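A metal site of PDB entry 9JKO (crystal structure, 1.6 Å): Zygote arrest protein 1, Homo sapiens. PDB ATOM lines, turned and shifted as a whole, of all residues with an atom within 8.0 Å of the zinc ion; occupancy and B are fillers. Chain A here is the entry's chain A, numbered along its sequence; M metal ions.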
ATOM      1  N   SER A  23     -29.390  -6.908 -18.544  1.00  0.00           N
ATOM      2  CA  SER A  23     -28.351  -6.002 -18.065  1.00  0.00           C
ATOM      3  C   SER A  23     -27.629  -5.398 -19.256  1.00  0.00           C
ATOM      4  O   SER A  23     -27.317  -6.101 -20.226  1.00  0.00           O
ATOM      5  CB  SER A  23     -27.327  -6.731 -17.182  1.00  0.00           C
ATOM      6  OG  SER A  23     -26.237  -5.873 -16.799  1.00  0.00           O
ATOM      7  N   TYR A  25     -24.677  -4.223 -18.716  1.00  0.00           N
ATOM      8  CA  TYR A  25     -23.283  -4.220 -18.240  1.00  0.00           C
ATOM      9  C   TYR A  25     -22.760  -5.645 -18.186  1.00  0.00           C
ATOM     10  O   TYR A  25     -22.191  -6.091 -17.195  1.00  0.00           O
ATOM     11  CB  TYR A  25     -23.182  -3.563 -16.862  1.00  0.00           C
ATOM     12  CG  TYR A  25     -23.288  -2.062 -16.940  1.00  0.00           C
ATOM     13  CD1 TYR A  25     -22.168  -1.296 -17.196  1.00  0.00           C
ATOM     14  CD2 TYR A  25     -24.536  -1.424 -16.809  1.00  0.00           C
ATOM     15  CE1 TYR A  25     -22.247   0.083 -17.284  1.00  0.00           C
ATOM     16  CE2 TYR A  25     -24.626  -0.032 -16.911  1.00  0.00           C
ATOM     17  CZ  TYR A  25     -23.474   0.714 -17.146  1.00  0.00           C
ATOM     18  OH  TYR A  25     -23.586   2.089 -17.274  1.00  0.00           O
ATOM     19  N   VAL A  26     -22.969  -6.401 -19.259  1.00  0.00           N
ATOM     20  CA  VAL A  26     -22.409  -7.737 -19.363  1.00  0.00           C
ATOM     21  C   VAL A  26     -21.014  -7.588 -19.950  1.00  0.00           C
ATOM     22  O   VAL A  26     -20.857  -7.067 -21.065  1.00  0.00           O
ATOM     23  CB  VAL A  26     -23.299  -8.656 -20.205  1.00  0.00           C
ATOM     24  CG1 VAL A  26     -22.645 -10.045 -20.380  1.00  0.00           C
ATOM     25  CG2 VAL A  26     -24.692  -8.795 -19.524  1.00  0.00           C
ATOM     26  N   TRP A  27     -20.008  -8.011 -19.202  1.00  0.00           N
ATOM     27  CA  TRP A  27     -18.618  -7.781 -19.571  1.00  0.00           C
ATOM     28  C   TRP A  27     -18.094  -9.004 -20.326  1.00  0.00           C
ATOM     29  O   TRP A  27     -17.990 -10.095 -19.751  1.00  0.00           O
ATOM     30  CB  TRP A  27     -17.791  -7.527 -18.314  1.00  0.00           C
ATOM     31  CG  TRP A  27     -18.200  -6.259 -17.656  1.00  0.00           C
ATOM     32  CD1 TRP A  27     -18.900  -6.098 -16.484  1.00  0.00           C
ATOM     33  CD2 TRP A  27     -17.976  -4.962 -18.181  1.00  0.00           C
ATOM     34  NE1 TRP A  27     -19.080  -4.745 -16.242  1.00  0.00           N
ATOM     35  CE2 TRP A  27     -18.531  -4.042 -17.274  1.00  0.00           C
ATOM     36  CE3 TRP A  27     -17.325  -4.489 -19.346  1.00  0.00           C
ATOM     37  CZ2 TRP A  27     -18.449  -2.648 -17.463  1.00  0.00           C
ATOM     38  CZ3 TRP A  27     -17.236  -3.116 -19.530  1.00  0.00           C
ATOM     39  CH2 TRP A  27     -17.814  -2.207 -18.598  1.00  0.00           C
ATOM     40  N   PHE A  37     -17.538 -11.883 -16.304  1.00  0.00           N
ATOM     41  CA  PHE A  37     -18.033 -11.739 -14.945  1.00  0.00           C
ATOM     42  C   PHE A  37     -19.454 -12.260 -14.835  1.00  0.00           C
ATOM     43  O   PHE A  37     -20.286 -11.987 -15.694  1.00  0.00           O
ATOM     44  CB  PHE A  37     -18.019 -10.273 -14.492  1.00  0.00           C
ATOM     45  CG  PHE A  37     -16.629  -9.758 -14.212  1.00  0.00           C
ATOM     46  CD1 PHE A  37     -15.911 -10.252 -13.120  1.00  0.00           C
ATOM     47  CD2 PHE A  37     -16.049  -8.773 -15.006  1.00  0.00           C
ATOM     48  CE1 PHE A  37     -14.636  -9.779 -12.848  1.00  0.00           C
ATOM     49  CE2 PHE A  37     -14.764  -8.312 -14.719  1.00  0.00           C
ATOM     50  CZ  PHE A  37     -14.074  -8.821 -13.634  1.00  0.00           C
ATOM     51  N   LYS A  38     -19.713 -12.960 -13.740  1.00  0.00           N
ATOM     52  CA  LYS A  38     -21.051 -13.426 -13.434  1.00  0.00           C
ATOM     53  C   LYS A  38     -21.939 -12.302 -12.920  1.00  0.00           C
ATOM     54  O   LYS A  38     -21.469 -11.263 -12.464  1.00  0.00           O
ATOM     55  CB  LYS A  38     -21.031 -14.555 -12.387  1.00  0.00           C
ATOM     56  CG  LYS A  38     -20.182 -15.717 -12.867  1.00  0.00           C
ATOM     57  CD  LYS A  38     -21.030 -16.632 -13.729  1.00  0.00           C
ATOM     58  CE  LYS A  38     -20.309 -17.918 -14.064  1.00  0.00           C
ATOM     59  NZ  LYS A  38     -20.233 -18.814 -12.892  1.00  0.00           N
ATOM     60  N   GLN A  39     -23.254 -12.560 -12.988  1.00  0.00           N
ATOM     61  CA  GLN A  39     -24.244 -11.762 -12.276  1.00  0.00           C
ATOM     62  C   GLN A  39     -25.018 -12.727 -11.394  1.00  0.00           C
ATOM     63  O   GLN A  39     -25.049 -13.929 -11.652  1.00  0.00           O
ATOM     64  CB  GLN A  39     -25.175 -11.014 -13.229  1.00  0.00           C
ATOM     65  CG  GLN A  39     -24.429  -9.843 -13.923  1.00  0.00           C
ATOM     66  CD  GLN A  39     -25.361  -8.888 -14.679  1.00  0.00           C
ATOM     67  OE1 GLN A  39     -26.586  -9.014 -14.632  1.00  0.00           O
ATOM     68  NE2 GLN A  39     -24.758  -7.919 -15.350  1.00  0.00           N
ATOM     69  N   HIS A  81     -28.325  -0.374 -12.411  1.00  0.00           N
ATOM     70  CA  HIS A  81     -27.419  -1.514 -12.427  1.00  0.00           C
ATOM     71  C   HIS A  81     -27.295  -2.010 -10.983  1.00  0.00           C
ATOM     72  O   HIS A  81     -26.893  -1.242 -10.096  1.00  0.00           O
ATOM     73  CB  HIS A  81     -26.044  -1.060 -12.961  1.00  0.00           C
ATOM     74  CG  HIS A  81     -24.961  -2.088 -12.907  1.00  0.00           C
ATOM     75  ND1 HIS A  81     -25.059  -3.340 -13.492  1.00  0.00           N
ATOM     76  CD2 HIS A  81     -23.737  -2.035 -12.329  1.00  0.00           C
ATOM     77  CE1 HIS A  81     -23.939  -4.009 -13.280  1.00  0.00           C
ATOM     78  NE2 HIS A  81     -23.116  -3.239 -12.576  1.00  0.00           N
ATOM     79  N   ARG A  82     -27.616  -3.295 -10.739  1.00  0.00           N
ATOM     80  CA  ARG A  82     -27.544  -3.827  -9.369  1.00  0.00           C
ATOM     81  C   ARG A  82     -26.107  -4.142  -9.001  1.00  0.00           C
ATOM     82  O   ARG A  82     -25.592  -5.240  -9.270  1.00  0.00           O
ATOM     83  CB  ARG A  82     -28.427  -5.051  -9.169  1.00  0.00           C
ATOM     84  CG  ARG A  82     -29.899  -4.745  -9.368  1.00  0.00           C
ATOM     85  CD  ARG A  82     -30.560  -4.413  -8.005  1.00  0.00           C
ATOM     86  NE  ARG A  82     -30.125  -5.194  -6.836  1.00  0.00           N
ATOM     87  CZ  ARG A  82     -31.012  -5.941  -6.190  1.00  0.00           C
ATOM     88  NH1 ARG A  82     -32.245  -6.102  -6.653  1.00  0.00           N
ATOM     89  NH2 ARG A  82     -30.634  -6.586  -5.085  1.00  0.00           N
ATOM     90  N   GLN A  83     -25.461  -3.149  -8.363  1.00  0.00           N
ATOM     91  CA  GLN A  83     -24.065  -3.304  -7.962  1.00  0.00           C
ATOM     92  C   GLN A  83     -23.871  -4.528  -7.105  1.00  0.00           C
ATOM     93  O   GLN A  83     -22.884  -5.259  -7.270  1.00  0.00           O
ATOM     94  CB  GLN A  83     -23.593  -2.066  -7.193  1.00  0.00           C
ATOM     95  CG  GLN A  83     -22.101  -2.133  -6.953  1.00  0.00           C
ATOM     96  CD  GLN A  83     -21.573  -0.994  -6.167  1.00  0.00           C
ATOM     97  OE1 GLN A  83     -22.282  -0.038  -5.854  1.00  0.00           O
ATOM     98  NE2 GLN A  83     -20.265  -0.977  -6.032  1.00  0.00           N
ATOM     99  N   ASP A  84     -24.824  -4.801  -6.229  1.00  0.00           N
ATOM    100  CA  ASP A  84     -24.714  -5.902  -5.295  1.00  0.00           C
ATOM    101  C   ASP A  84     -24.838  -7.268  -5.959  1.00  0.00           C
ATOM    102  O   ASP A  84     -24.414  -8.254  -5.357  1.00  0.00           O
ATOM    103  CB  ASP A  84     -25.765  -5.722  -4.206  1.00  0.00           C
ATOM    104  CG  ASP A  84     -27.179  -5.697  -4.743  1.00  0.00           C
ATOM    105  OD1 ASP A  84     -27.470  -4.961  -5.719  1.00  0.00           O
ATOM    106  OD2 ASP A  84     -28.021  -6.394  -4.152  1.00  0.00           O
ATOM    107  N   LEU A  85     -25.323  -7.322  -7.214  1.00  0.00           N
ATOM    108  CA  LEU A  85     -25.504  -8.549  -7.973  1.00  0.00           C
ATOM    109  C   LEU A  85     -24.540  -8.658  -9.148  1.00  0.00           C
ATOM    110  O   LEU A  85     -24.729  -9.492 -10.028  1.00  0.00           O
ATOM    111  CB  LEU A  85     -26.951  -8.638  -8.465  1.00  0.00           C
ATOM    112  CG  LEU A  85     -27.992  -8.500  -7.358  1.00  0.00           C
ATOM    113  CD1 LEU A  85     -29.382  -8.502  -7.948  1.00  0.00           C
ATOM    114  CD2 LEU A  85     -27.846  -9.639  -6.315  1.00  0.00           C
ATOM    115  N   CYS A  86     -23.518  -7.803  -9.192  1.00  0.00           N
ATOM    116  CA  CYS A  86     -22.608  -7.709 -10.343  1.00  0.00           C
ATOM    117  C   CYS A  86     -21.250  -8.300  -9.966  1.00  0.00           C
ATOM    118  O   CYS A  86     -20.607  -7.829  -9.028  1.00  0.00           O
ATOM    119  CB  CYS A  86     -22.428  -6.258 -10.773  1.00  0.00           C
ATOM    120  SG  CYS A  86     -21.203  -6.076 -12.105  1.00  0.00           S
ATOM    121  N   GLY A  87     -20.791  -9.307 -10.712  1.00  0.00           N
ATOM    122  CA  GLY A  87     -19.507  -9.912 -10.408  1.00  0.00           C
ATOM    123  C   GLY A  87     -18.357  -8.937 -10.575  1.00  0.00           C
ATOM    124  O   GLY A  87     -17.313  -9.087  -9.921  1.00  0.00           O
ATOM    125  N   ARG A  88     -18.528  -7.919 -11.423  1.00  0.00           N
ATOM    126  CA  ARG A  88     -17.407  -6.982 -11.615  1.00  0.00           C
ATOM    127  C   ARG A  88     -17.288  -5.982 -10.470  1.00  0.00           C
ATOM    128  O   ARG A  88     -16.168  -5.694 -10.033  1.00  0.00           O
ATOM    129  CB  ARG A  88     -17.520  -6.222 -12.929  1.00  0.00           C
ATOM    130  CG  ARG A  88     -16.318  -5.257 -13.174  1.00  0.00           C
ATOM    131  CD  ARG A  88     -15.910  -5.161 -14.628  1.00  0.00           C
ATOM    132  NE  ARG A  88     -14.616  -4.495 -14.791  1.00  0.00           N
ATOM    133  CZ  ARG A  88     -14.234  -3.831 -15.878  1.00  0.00           C
ATOM    134  NH1 ARG A  88     -15.013  -3.754 -16.961  1.00  0.00           N
ATOM    135  NH2 ARG A  88     -13.019  -3.291 -15.914  1.00  0.00           N
ATOM    136  N   CYS A  89     -18.414  -5.393  -9.994  1.00  0.00           N
ATOM    137  CA  CYS A  89     -18.329  -4.253  -9.075  1.00  0.00           C
ATOM    138  C   CYS A  89     -18.944  -4.447  -7.691  1.00  0.00           C
ATOM    139  O   CYS A  89     -18.907  -3.506  -6.898  1.00  0.00           O
ATOM    140  CB  CYS A  89     -18.943  -2.983  -9.702  1.00  0.00           C
ATOM    141  SG  CYS A  89     -20.774  -2.963  -9.962  1.00  0.00           S
ATOM    142  N   LYS A  90     -19.457  -5.632  -7.347  1.00  0.00           N
ATOM    143  CA  LYS A  90     -20.079  -5.777  -6.043  1.00  0.00           C
ATOM    144  C   LYS A  90     -19.092  -5.544  -4.905  1.00  0.00           C
ATOM    145  O   LYS A  90     -19.522  -5.140  -3.819  1.00  0.00           O
ATOM    146  CB  LYS A  90     -20.753  -7.162  -5.922  1.00  0.00           C
ATOM    147  CG  LYS A  90     -19.808  -8.352  -5.941  1.00  0.00           C
ATOM    148  CD  LYS A  90     -20.590  -9.649  -6.060  1.00  0.00           C
ATOM    149  CE  LYS A  90     -19.777 -10.839  -5.646  1.00  0.00           C
ATOM    150  NZ  LYS A  90     -18.432 -10.844  -6.282  1.00  0.00           N
ATOM    151  N   GLY A  91     -17.804  -5.745  -5.128  1.00  0.00           N
ATOM    152  CA  GLY A  91     -16.772  -5.521  -4.122  1.00  0.00           C
ATOM    153  C   GLY A  91     -16.087  -4.176  -4.152  1.00  0.00           C
ATOM    154  O   GLY A  91     -15.186  -3.935  -3.333  1.00  0.00           O
ATOM    155  N   LYS A  92     -16.509  -3.276  -5.016  1.00  0.00           N
ATOM    156  CA  LYS A  92     -15.794  -2.025  -5.247  1.00  0.00           C
ATOM    157  C   LYS A  92     -16.611  -0.840  -4.751  1.00  0.00           C
ATOM    158  O   LYS A  92     -17.822  -0.931  -4.577  1.00  0.00           O
ATOM    159  CB  LYS A  92     -15.521  -1.903  -6.743  1.00  0.00           C
ATOM    160  CG  LYS A  92     -14.373  -2.778  -7.232  1.00  0.00           C
ATOM    161  CD  LYS A  92     -14.525  -3.328  -8.616  1.00  0.00           C
ATOM    162  CE  LYS A  92     -13.258  -3.280  -9.365  1.00  0.00           C
ATOM    163  NZ  LYS A  92     -12.066  -4.005  -8.811  1.00  0.00           N
ATOM    164  N   LEU A  94     -17.114   2.063  -6.424  1.00  0.00           N
ATOM    165  CA  LEU A  94     -17.840   2.683  -7.543  1.00  0.00           C
ATOM    166  C   LEU A  94     -18.391   1.600  -8.458  1.00  0.00           C
ATOM    167  O   LEU A  94     -17.638   0.740  -8.927  1.00  0.00           O
ATOM    168  CB  LEU A  94     -16.910   3.621  -8.325  1.00  0.00           C
ATOM    169  CG  LEU A  94     -16.407   4.825  -7.533  1.00  0.00           C
ATOM    170  CD1 LEU A  94     -15.675   5.680  -8.519  1.00  0.00           C
ATOM    171  CD2 LEU A  94     -17.516   5.642  -6.921  1.00  0.00           C
ATOM    172  N   SER A  95     -19.690   1.622  -8.700  1.00  0.00           N
ATOM    173  CA  SER A  95     -20.297   0.616  -9.576  1.00  0.00           C
ATOM    174  C   SER A  95     -19.876   0.826 -11.029  1.00  0.00           C
ATOM    175  O   SER A  95     -19.339   1.884 -11.424  1.00  0.00           O
ATOM    176  CB  SER A  95     -21.817   0.698  -9.491  1.00  0.00           C
ATOM    177  OG  SER A  95     -22.225   2.033  -9.762  1.00  0.00           O
ATOM    178  N   CYS A  96     -20.164  -0.188 -11.864  1.00  0.00           N
ATOM    179  CA  CYS A  96     -19.922  -0.101 -13.302  1.00  0.00           C
ATOM    180  C   CYS A  96     -20.596   1.114 -13.920  1.00  0.00           C
ATOM    181  O   CYS A  96     -20.105   1.657 -14.919  1.00  0.00           O
ATOM    182  CB  CYS A  96     -20.428  -1.355 -14.027  1.00  0.00           C
ATOM    183  SG  CYS A  96     -19.584  -2.904 -13.573  1.00  0.00           S
ATOM    184  N   ASP A  97     -21.753   1.516 -13.400  1.00  0.00           N
ATOM    185  CA  ASP A  97     -22.549   2.579 -13.993  1.00  0.00           C
ATOM    186  C   ASP A  97     -22.362   3.903 -13.264  1.00  0.00           C
ATOM    187  O   ASP A  97     -23.165   4.824 -13.466  1.00  0.00           O
ATOM    188  CB  ASP A  97     -24.033   2.199 -14.033  1.00  0.00           C
ATOM    189  CG  ASP A  97     -24.658   2.113 -12.643  1.00  0.00           C
ATOM    190  OD1 ASP A  97     -24.014   1.603 -11.707  1.00  0.00           O
ATOM    191  OD2 ASP A  97     -25.801   2.575 -12.482  1.00  0.00           O
ATOM    192  N   SER A  98     -21.329   4.001 -12.432  1.00  0.00           N
ATOM    193  CA  SER A  98     -21.032   5.212 -11.669  1.00  0.00           C
ATOM    194  C   SER A  98     -20.365   6.265 -12.540  1.00  0.00           C
ATOM    195  O   SER A  98     -20.187   7.403 -12.075  1.00  0.00           O
ATOM    196  CB  SER A  98     -20.118   4.889 -10.477  1.00  0.00           C
ATOM    197  OG  SER A  98     -20.870   4.388  -9.391  1.00  0.00           O
ATOM    198  OXT SER A  98     -19.997   6.031 -13.705  1.00  0.00           O
HETATM  199 ZN    ZN M   1     -21.131  -3.754 -12.079  1.00  0.00          ZN
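The zinc ion is bound by a ring nitrogen (NE2) of His 81 (2.1 Å), the side-chain sulfur of Cys 89 (2.3 Å), the side-chain sulfur of Cys 96 (2.3 Å) and the side-chain sulfur of Cys 86 (2.3 Å).
The backbone carbonyl oxygen (O) of Cys 89 sits at hydrogen-bond distance from the side-chain amide nitrogen (NE2) of Gln 83.
The side-chain sulfur (SG) of Cys 96 lies close to the indole nitrogen (NE1) of Trp 27, at 3.3 Å.
The side-chain sulfur (SG) of Cys 86 lies close to the backbone NH (N) of Arg 88 (3.3 Å).
Within 4 Å of the zinc ion: His 81, Cys 86, Cys 89 and Cys 96.
The nearest printed residue that does not touch the zinc ion is Arg 88 (4.5 Å).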
